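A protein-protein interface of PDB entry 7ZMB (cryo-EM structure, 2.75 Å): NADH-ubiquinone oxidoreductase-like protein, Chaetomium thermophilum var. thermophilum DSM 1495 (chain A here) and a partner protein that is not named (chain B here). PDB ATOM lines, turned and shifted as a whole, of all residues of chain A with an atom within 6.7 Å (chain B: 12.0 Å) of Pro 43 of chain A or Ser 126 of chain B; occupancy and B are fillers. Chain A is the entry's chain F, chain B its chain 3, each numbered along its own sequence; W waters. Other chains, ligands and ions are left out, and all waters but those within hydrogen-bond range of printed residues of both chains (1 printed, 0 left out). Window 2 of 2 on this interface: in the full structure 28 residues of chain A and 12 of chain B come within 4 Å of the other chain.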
ATOM      1  N   VAL A  29      -5.634 -29.241  22.550  1.00  0.00           N
ATOM      2  CA  VAL A  29      -5.037 -29.495  21.242  1.00  0.00           C
ATOM      3  C   VAL A  29      -3.853 -28.548  21.068  1.00  0.00           C
ATOM      4  O   VAL A  29      -4.066 -27.337  20.916  1.00  0.00           O
ATOM      5  CB  VAL A  29      -6.057 -29.314  20.113  1.00  0.00           C
ATOM      6  CG1 VAL A  29      -5.521 -29.913  18.831  1.00  0.00           C
ATOM      7  CG2 VAL A  29      -7.387 -29.943  20.495  1.00  0.00           C
ATOM      8  N   PRO A  30      -2.616 -29.045  21.039  1.00  0.00           N
ATOM      9  CA  PRO A  30      -1.456 -28.146  21.003  1.00  0.00           C
ATOM     10  C   PRO A  30      -1.502 -27.201  19.814  1.00  0.00           C
ATOM     11  O   PRO A  30      -1.787 -27.602  18.683  1.00  0.00           O
ATOM     12  CB  PRO A  30      -0.270 -29.109  20.909  1.00  0.00           C
ATOM     13  CG  PRO A  30      -0.762 -30.360  21.497  1.00  0.00           C
ATOM     14  CD  PRO A  30      -2.208 -30.455  21.112  1.00  0.00           C
ATOM     15  N   GLY A  31      -1.226 -25.932  20.081  1.00  0.00           N
ATOM     16  CA  GLY A  31      -1.273 -24.922  19.054  1.00  0.00           C
ATOM     17  C   GLY A  31      -2.641 -24.363  18.753  1.00  0.00           C
ATOM     18  O   GLY A  31      -2.744 -23.444  17.933  1.00  0.00           O
ATOM     19  N   GLY A  40      -0.674 -20.022  21.746  1.00  0.00           N
ATOM     20  CA  GLY A  40      -1.283 -21.281  21.391  1.00  0.00           C
ATOM     21  C   GLY A  40      -1.249 -22.249  22.558  1.00  0.00           C
ATOM     22  O   GLY A  40      -0.672 -21.988  23.606  1.00  0.00           O
ATOM     23  N   THR A  41      -1.883 -23.390  22.352  1.00  0.00           N
ATOM     24  CA  THR A  41      -1.946 -24.401  23.392  1.00  0.00           C
ATOM     25  C   THR A  41      -0.618 -25.138  23.475  1.00  0.00           C
ATOM     26  O   THR A  41      -0.116 -25.646  22.472  1.00  0.00           O
ATOM     27  CB  THR A  41      -3.093 -25.358  23.105  1.00  0.00           C
ATOM     28  OG1 THR A  41      -4.255 -24.590  22.775  1.00  0.00           O
ATOM     29  CG2 THR A  41      -3.403 -26.186  24.309  1.00  0.00           C
ATOM     30  N   HIS A  42      -0.047 -25.137  24.683  1.00  0.00           N
ATOM     31  CA  HIS A  42       1.291 -25.740  24.912  1.00  0.00           C
ATOM     32  C   HIS A  42       1.266 -27.267  24.745  1.00  0.00           C
ATOM     33  O   HIS A  42       0.505 -27.906  25.473  1.00  0.00           O
ATOM     34  CB  HIS A  42       1.849 -25.345  26.284  1.00  0.00           C
ATOM     35  CG  HIS A  42       3.334 -25.460  26.367  1.00  0.00           C
ATOM     36  ND1 HIS A  42       4.166 -24.368  26.240  1.00  0.00           N
ATOM     37  CD2 HIS A  42       4.139 -26.527  26.548  1.00  0.00           C
ATOM     38  CE1 HIS A  42       5.418 -24.756  26.351  1.00  0.00           C
ATOM     39  NE2 HIS A  42       5.428 -26.076  26.537  1.00  0.00           N
ATOM     40  N   PRO A  43       2.113 -27.883  23.884  1.00  0.00           N
ATOM     41  CA  PRO A  43       2.104 -29.341  23.714  1.00  0.00           C
ATOM     42  C   PRO A  43       2.333 -30.123  24.987  1.00  0.00           C
ATOM     43  O   PRO A  43       1.989 -31.307  25.024  1.00  0.00           O
ATOM     44  CB  PRO A  43       3.234 -29.579  22.706  1.00  0.00           C
ATOM     45  CG  PRO A  43       4.067 -28.335  22.767  1.00  0.00           C
ATOM     46  CD  PRO A  43       3.103 -27.239  23.014  1.00  0.00           C
ATOM     47  N   SER A  44       2.921 -29.520  26.014  1.00  0.00           N
ATOM     48  CA  SER A  44       3.255 -30.289  27.242  1.00  0.00           C
ATOM     49  C   SER A  44       3.389 -29.296  28.399  1.00  0.00           C
ATOM     50  O   SER A  44       4.524 -29.089  28.848  1.00  0.00           O
ATOM     51  CB  SER A  44       4.527 -31.088  27.056  1.00  0.00           C
ATOM     52  OG  SER A  44       5.646 -30.248  26.820  1.00  0.00           O
ATOM     53  N   PRO A  45       2.307 -28.704  28.962  1.00  0.00           N
ATOM     54  CA  PRO A  45       2.498 -27.623  29.940  1.00  0.00           C
ATOM     55  C   PRO A  45       3.066 -28.055  31.286  1.00  0.00           C
ATOM     56  O   PRO A  45       3.766 -27.255  31.912  1.00  0.00           O
ATOM     57  CB  PRO A  45       1.084 -27.046  30.087  1.00  0.00           C
ATOM     58  CG  PRO A  45       0.200 -28.172  29.757  1.00  0.00           C
ATOM     59  CD  PRO A  45       0.885 -28.917  28.663  1.00  0.00           C
ATOM     60  N   LYS A 145       7.771 -32.093  12.128  1.00  0.00           N
ATOM     61  CA  LYS A 145       6.626 -31.206  11.975  1.00  0.00           C
ATOM     62  C   LYS A 145       5.546 -31.841  11.108  1.00  0.00           C
ATOM     63  O   LYS A 145       5.830 -32.434  10.064  1.00  0.00           O
ATOM     64  CB  LYS A 145       7.069 -29.876  11.368  1.00  0.00           C
ATOM     65  CG  LYS A 145       7.967 -29.055  12.277  1.00  0.00           C
ATOM     66  CD  LYS A 145       8.330 -27.724  11.642  1.00  0.00           C
ATOM     67  CE  LYS A 145       9.294 -26.938  12.516  1.00  0.00           C
ATOM     68  NZ  LYS A 145       8.659 -26.491  13.785  1.00  0.00           N
ATOM     69  N   GLN A 201      -0.191 -36.900  29.383  1.00  0.00           N
ATOM     70  CA  GLN A 201      -0.508 -35.468  29.503  1.00  0.00           C
ATOM     71  C   GLN A 201      -1.670 -35.247  30.463  1.00  0.00           C
ATOM     72  O   GLN A 201      -2.274 -36.234  30.910  1.00  0.00           O
ATOM     73  CB  GLN A 201      -0.791 -34.929  28.105  1.00  0.00           C
ATOM     74  CG  GLN A 201       0.397 -35.031  27.164  1.00  0.00           C
ATOM     75  CD  GLN A 201       1.423 -33.963  27.450  1.00  0.00           C
ATOM     76  OE1 GLN A 201       1.086 -32.811  27.712  1.00  0.00           O
ATOM     77  NE2 GLN A 201       2.689 -34.342  27.397  1.00  0.00           N
ATOM     78  N   GLU A 220      -0.644 -21.381  29.711  1.00  0.00           N
ATOM     79  CA  GLU A 220       0.278 -20.839  28.725  1.00  0.00           C
ATOM     80  C   GLU A 220       0.814 -19.484  29.163  1.00  0.00           C
ATOM     81  O   GLU A 220       1.971 -19.156  28.891  1.00  0.00           O
ATOM     82  CB  GLU A 220      -0.408 -20.738  27.367  1.00  0.00           C
ATOM     83  CG  GLU A 220      -0.563 -22.064  26.678  1.00  0.00           C
ATOM     84  CD  GLU A 220      -1.683 -22.903  27.253  1.00  0.00           C
ATOM     85  OE1 GLU A 220      -1.801 -24.083  26.866  1.00  0.00           O
ATOM     86  OE2 GLU A 220      -2.444 -22.385  28.091  1.00  0.00           O
ATOM     87  N   LEU B 124       2.169 -23.941  11.915  1.00  0.00           N
ATOM     88  CA  LEU B 124       3.258 -23.234  12.576  1.00  0.00           C
ATOM     89  C   LEU B 124       2.957 -23.144  14.070  1.00  0.00           C
ATOM     90  O   LEU B 124       2.478 -22.122  14.554  1.00  0.00           O
ATOM     91  CB  LEU B 124       3.444 -21.840  11.956  1.00  0.00           C
ATOM     92  CG  LEU B 124       4.673 -20.978  12.275  1.00  0.00           C
ATOM     93  CD1 LEU B 124       4.991 -20.094  11.082  1.00  0.00           C
ATOM     94  CD2 LEU B 124       4.489 -20.114  13.512  1.00  0.00           C
ATOM     95  N   LYS B 125       3.217 -24.234  14.791  1.00  0.00           N
ATOM     96  CA  LYS B 125       2.956 -24.295  16.222  1.00  0.00           C
ATOM     97  C   LYS B 125       4.130 -24.985  16.903  1.00  0.00           C
ATOM     98  O   LYS B 125       5.040 -25.501  16.248  1.00  0.00           O
ATOM     99  CB  LYS B 125       1.632 -25.012  16.521  1.00  0.00           C
ATOM    100  CG  LYS B 125       0.428 -24.330  15.903  1.00  0.00           C
ATOM    101  CD  LYS B 125       0.238 -22.937  16.480  1.00  0.00           C
ATOM    102  CE  LYS B 125      -0.883 -22.199  15.773  1.00  0.00           C
ATOM    103  NZ  LYS B 125      -1.023 -20.801  16.260  1.00  0.00           N
ATOM    104  N   SER B 126       4.102 -24.990  18.234  1.00  0.00           N
ATOM    105  CA  SER B 126       5.195 -25.560  19.010  1.00  0.00           C
ATOM    106  C   SER B 126       5.339 -27.051  18.729  1.00  0.00           C
ATOM    107  O   SER B 126       4.356 -27.773  18.545  1.00  0.00           O
ATOM    108  CB  SER B 126       4.961 -25.334  20.504  1.00  0.00           C
ATOM    109  OG  SER B 126       5.993 -25.922  21.274  1.00  0.00           O
ATOM    110  N   SER B 127       6.590 -27.510  18.695  1.00  0.00           N
ATOM    111  CA  SER B 127       6.872 -28.919  18.454  1.00  0.00           C
ATOM    112  C   SER B 127       7.936 -29.450  19.405  1.00  0.00           C
ATOM    113  O   SER B 127       8.674 -30.379  19.055  1.00  0.00           O
ATOM    114  CB  SER B 127       7.308 -29.150  17.009  1.00  0.00           C
ATOM    115  OG  SER B 127       8.658 -28.766  16.826  1.00  0.00           O
ATOM    116  N   VAL B 128       8.040 -28.889  20.604  1.00  0.00           N
ATOM    117  CA  VAL B 128       9.027 -29.330  21.584  1.00  0.00           C
ATOM    118  C   VAL B 128       8.270 -29.782  22.825  1.00  0.00           C
ATOM    119  O   VAL B 128       7.709 -28.964  23.563  1.00  0.00           O
ATOM    120  CB  VAL B 128      10.056 -28.240  21.904  1.00  0.00           C
ATOM    121  CG1 VAL B 128      10.749 -28.519  23.195  1.00  0.00           C
ATOM    122  CG2 VAL B 128      11.072 -28.158  20.790  1.00  0.00           C
ATOM    123  N   VAL B 129       8.191 -31.100  22.986  1.00  0.00           N
ATOM    124  CA  VAL B 129       7.523 -31.688  24.178  1.00  0.00           C
ATOM    125  C   VAL B 129       8.597 -32.058  25.208  1.00  0.00           C
ATOM    126  O   VAL B 129       9.517 -32.811  24.856  1.00  0.00           O
ATOM    127  CB  VAL B 129       6.670 -32.909  23.782  1.00  0.00           C
ATOM    128  CG1 VAL B 129       6.246 -33.729  24.990  1.00  0.00           C
ATOM    129  CG2 VAL B 129       5.464 -32.512  22.949  1.00  0.00           C
ATOM    130  N   ILE B 130       8.493 -31.522  26.423  1.00  0.00           N
ATOM    131  CA  ILE B 130       9.431 -31.876  27.522  1.00  0.00           C
ATOM    132  C   ILE B 130       8.791 -33.005  28.322  1.00  0.00           C
ATOM    133  O   ILE B 130       7.570 -33.019  28.418  1.00  0.00           O
ATOM    134  CB  ILE B 130       9.738 -30.654  28.406  1.00  0.00           C
ATOM    135  CG1 ILE B 130      10.028 -29.413  27.559  1.00  0.00           C
ATOM    136  CG2 ILE B 130      10.873 -30.952  29.373  1.00  0.00           C
ATOM    137  CD1 ILE B 130      10.553 -28.247  28.353  1.00  0.00           C
ATOM    138  N   SER B 131       9.601 -33.917  28.858  1.00  0.00           N
ATOM    139  CA  SER B 131       9.073 -35.023  29.690  1.00  0.00           C
ATOM    140  C   SER B 131       9.780 -34.989  31.044  1.00  0.00           C
ATOM    141  O   SER B 131      10.936 -34.552  31.079  1.00  0.00           O
ATOM    142  CB  SER B 131       9.207 -36.351  28.990  1.00  0.00           C
ATOM    143  OG  SER B 131       8.269 -36.467  27.936  1.00  0.00           O
ATOM    144  N   TYR B 132       9.109 -35.414  32.112  1.00  0.00           N
ATOM    145  CA  TYR B 132       9.619 -35.342  33.474  1.00  0.00           C
ATOM    146  C   TYR B 132       9.760 -36.759  34.002  1.00  0.00           C
ATOM    147  O   TYR B 132       8.760 -37.460  34.180  1.00  0.00           O
ATOM    148  CB  TYR B 132       8.679 -34.518  34.357  1.00  0.00           C
ATOM    149  CG  TYR B 132       9.149 -34.266  35.770  1.00  0.00           C
ATOM    150  CD1 TYR B 132      10.349 -33.625  36.020  1.00  0.00           C
ATOM    151  CD2 TYR B 132       8.381 -34.663  36.857  1.00  0.00           C
ATOM    152  CE1 TYR B 132      10.780 -33.385  37.305  1.00  0.00           C
ATOM    153  CE2 TYR B 132       8.802 -34.428  38.150  1.00  0.00           C
ATOM    154  CZ  TYR B 132      10.006 -33.785  38.368  1.00  0.00           C
ATOM    155  OH  TYR B 132      10.433 -33.544  39.653  1.00  0.00           O
HETATM  156  O   HOH W   1       5.241 -33.927  28.916  1.00  0.00           O
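Hydrophobic or aromatic side chains of chain B that line the printed part of chain A: Val 129.
Hydrophobic or aromatic side chains of chain A within 4 Å of the printed part of chain B: Pro 43.
OG of Ser 44 of chain A is in hydrogen-bond range of N of Ile 130 of chain B.
Water W1 lies within hydrogen-bond range of O of Ile 130 of chain B and NE2 of Gln 201 of chain A.
N of Gly 31 of chain A lies within hydrogen-bond range of O of Thr 41 of chain A (2.7 Å).
O of Pro 43 of chain A sits close to OE1 of Gln 201 of chain A.
CE of Lys 125 of chain B touches O of Gly 31 of chain A (3.1 Å).
Ser 126 of chain B touches Pro 43 of chain A.
Pro 43 of chain A touches Val 128 of chain B (CG to O, 3.8 Å).
CB of Pro 43 of chain A touches CG2 of Val 129 of chain B, 3.7 Å away.
Ser 44 of chain A touches Val 129 of chain B (OG to CA, 3.5 Å).
Lys 145 of chain A touches Ser 127 of chain B (NZ to OG, 3.8 Å).
No residue of chain B comes within 4 Å of Pro 30 of chain A.
Gly 31 of chain A touches just one residue of chain B: Lys 125.
No residue of chain B comes within 4 Å of Gly 40 of chain A.
Ser 44 of chain A touches just these residues of chain B: Val 129 and Ile 130.
No residue of chain B comes within 4 Å of Pro 45 of chain A.
Of the printed residues of chain A, Lys 125 of chain B touches Gly 31 (3.1 Å).
Of the printed residues of chain A, Ser 127 of chain B touches Lys 145.
Of the printed residues of chain A, Val 128 of chain B touches Pro 43 (3.8 Å).
Printed residues of chain A within 4 Å of Val 129 of chain B: Pro 43 and Ser 44.
Of the printed residues of chain A, Ile 130 of chain B touches Ser 44 (3.1 Å).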
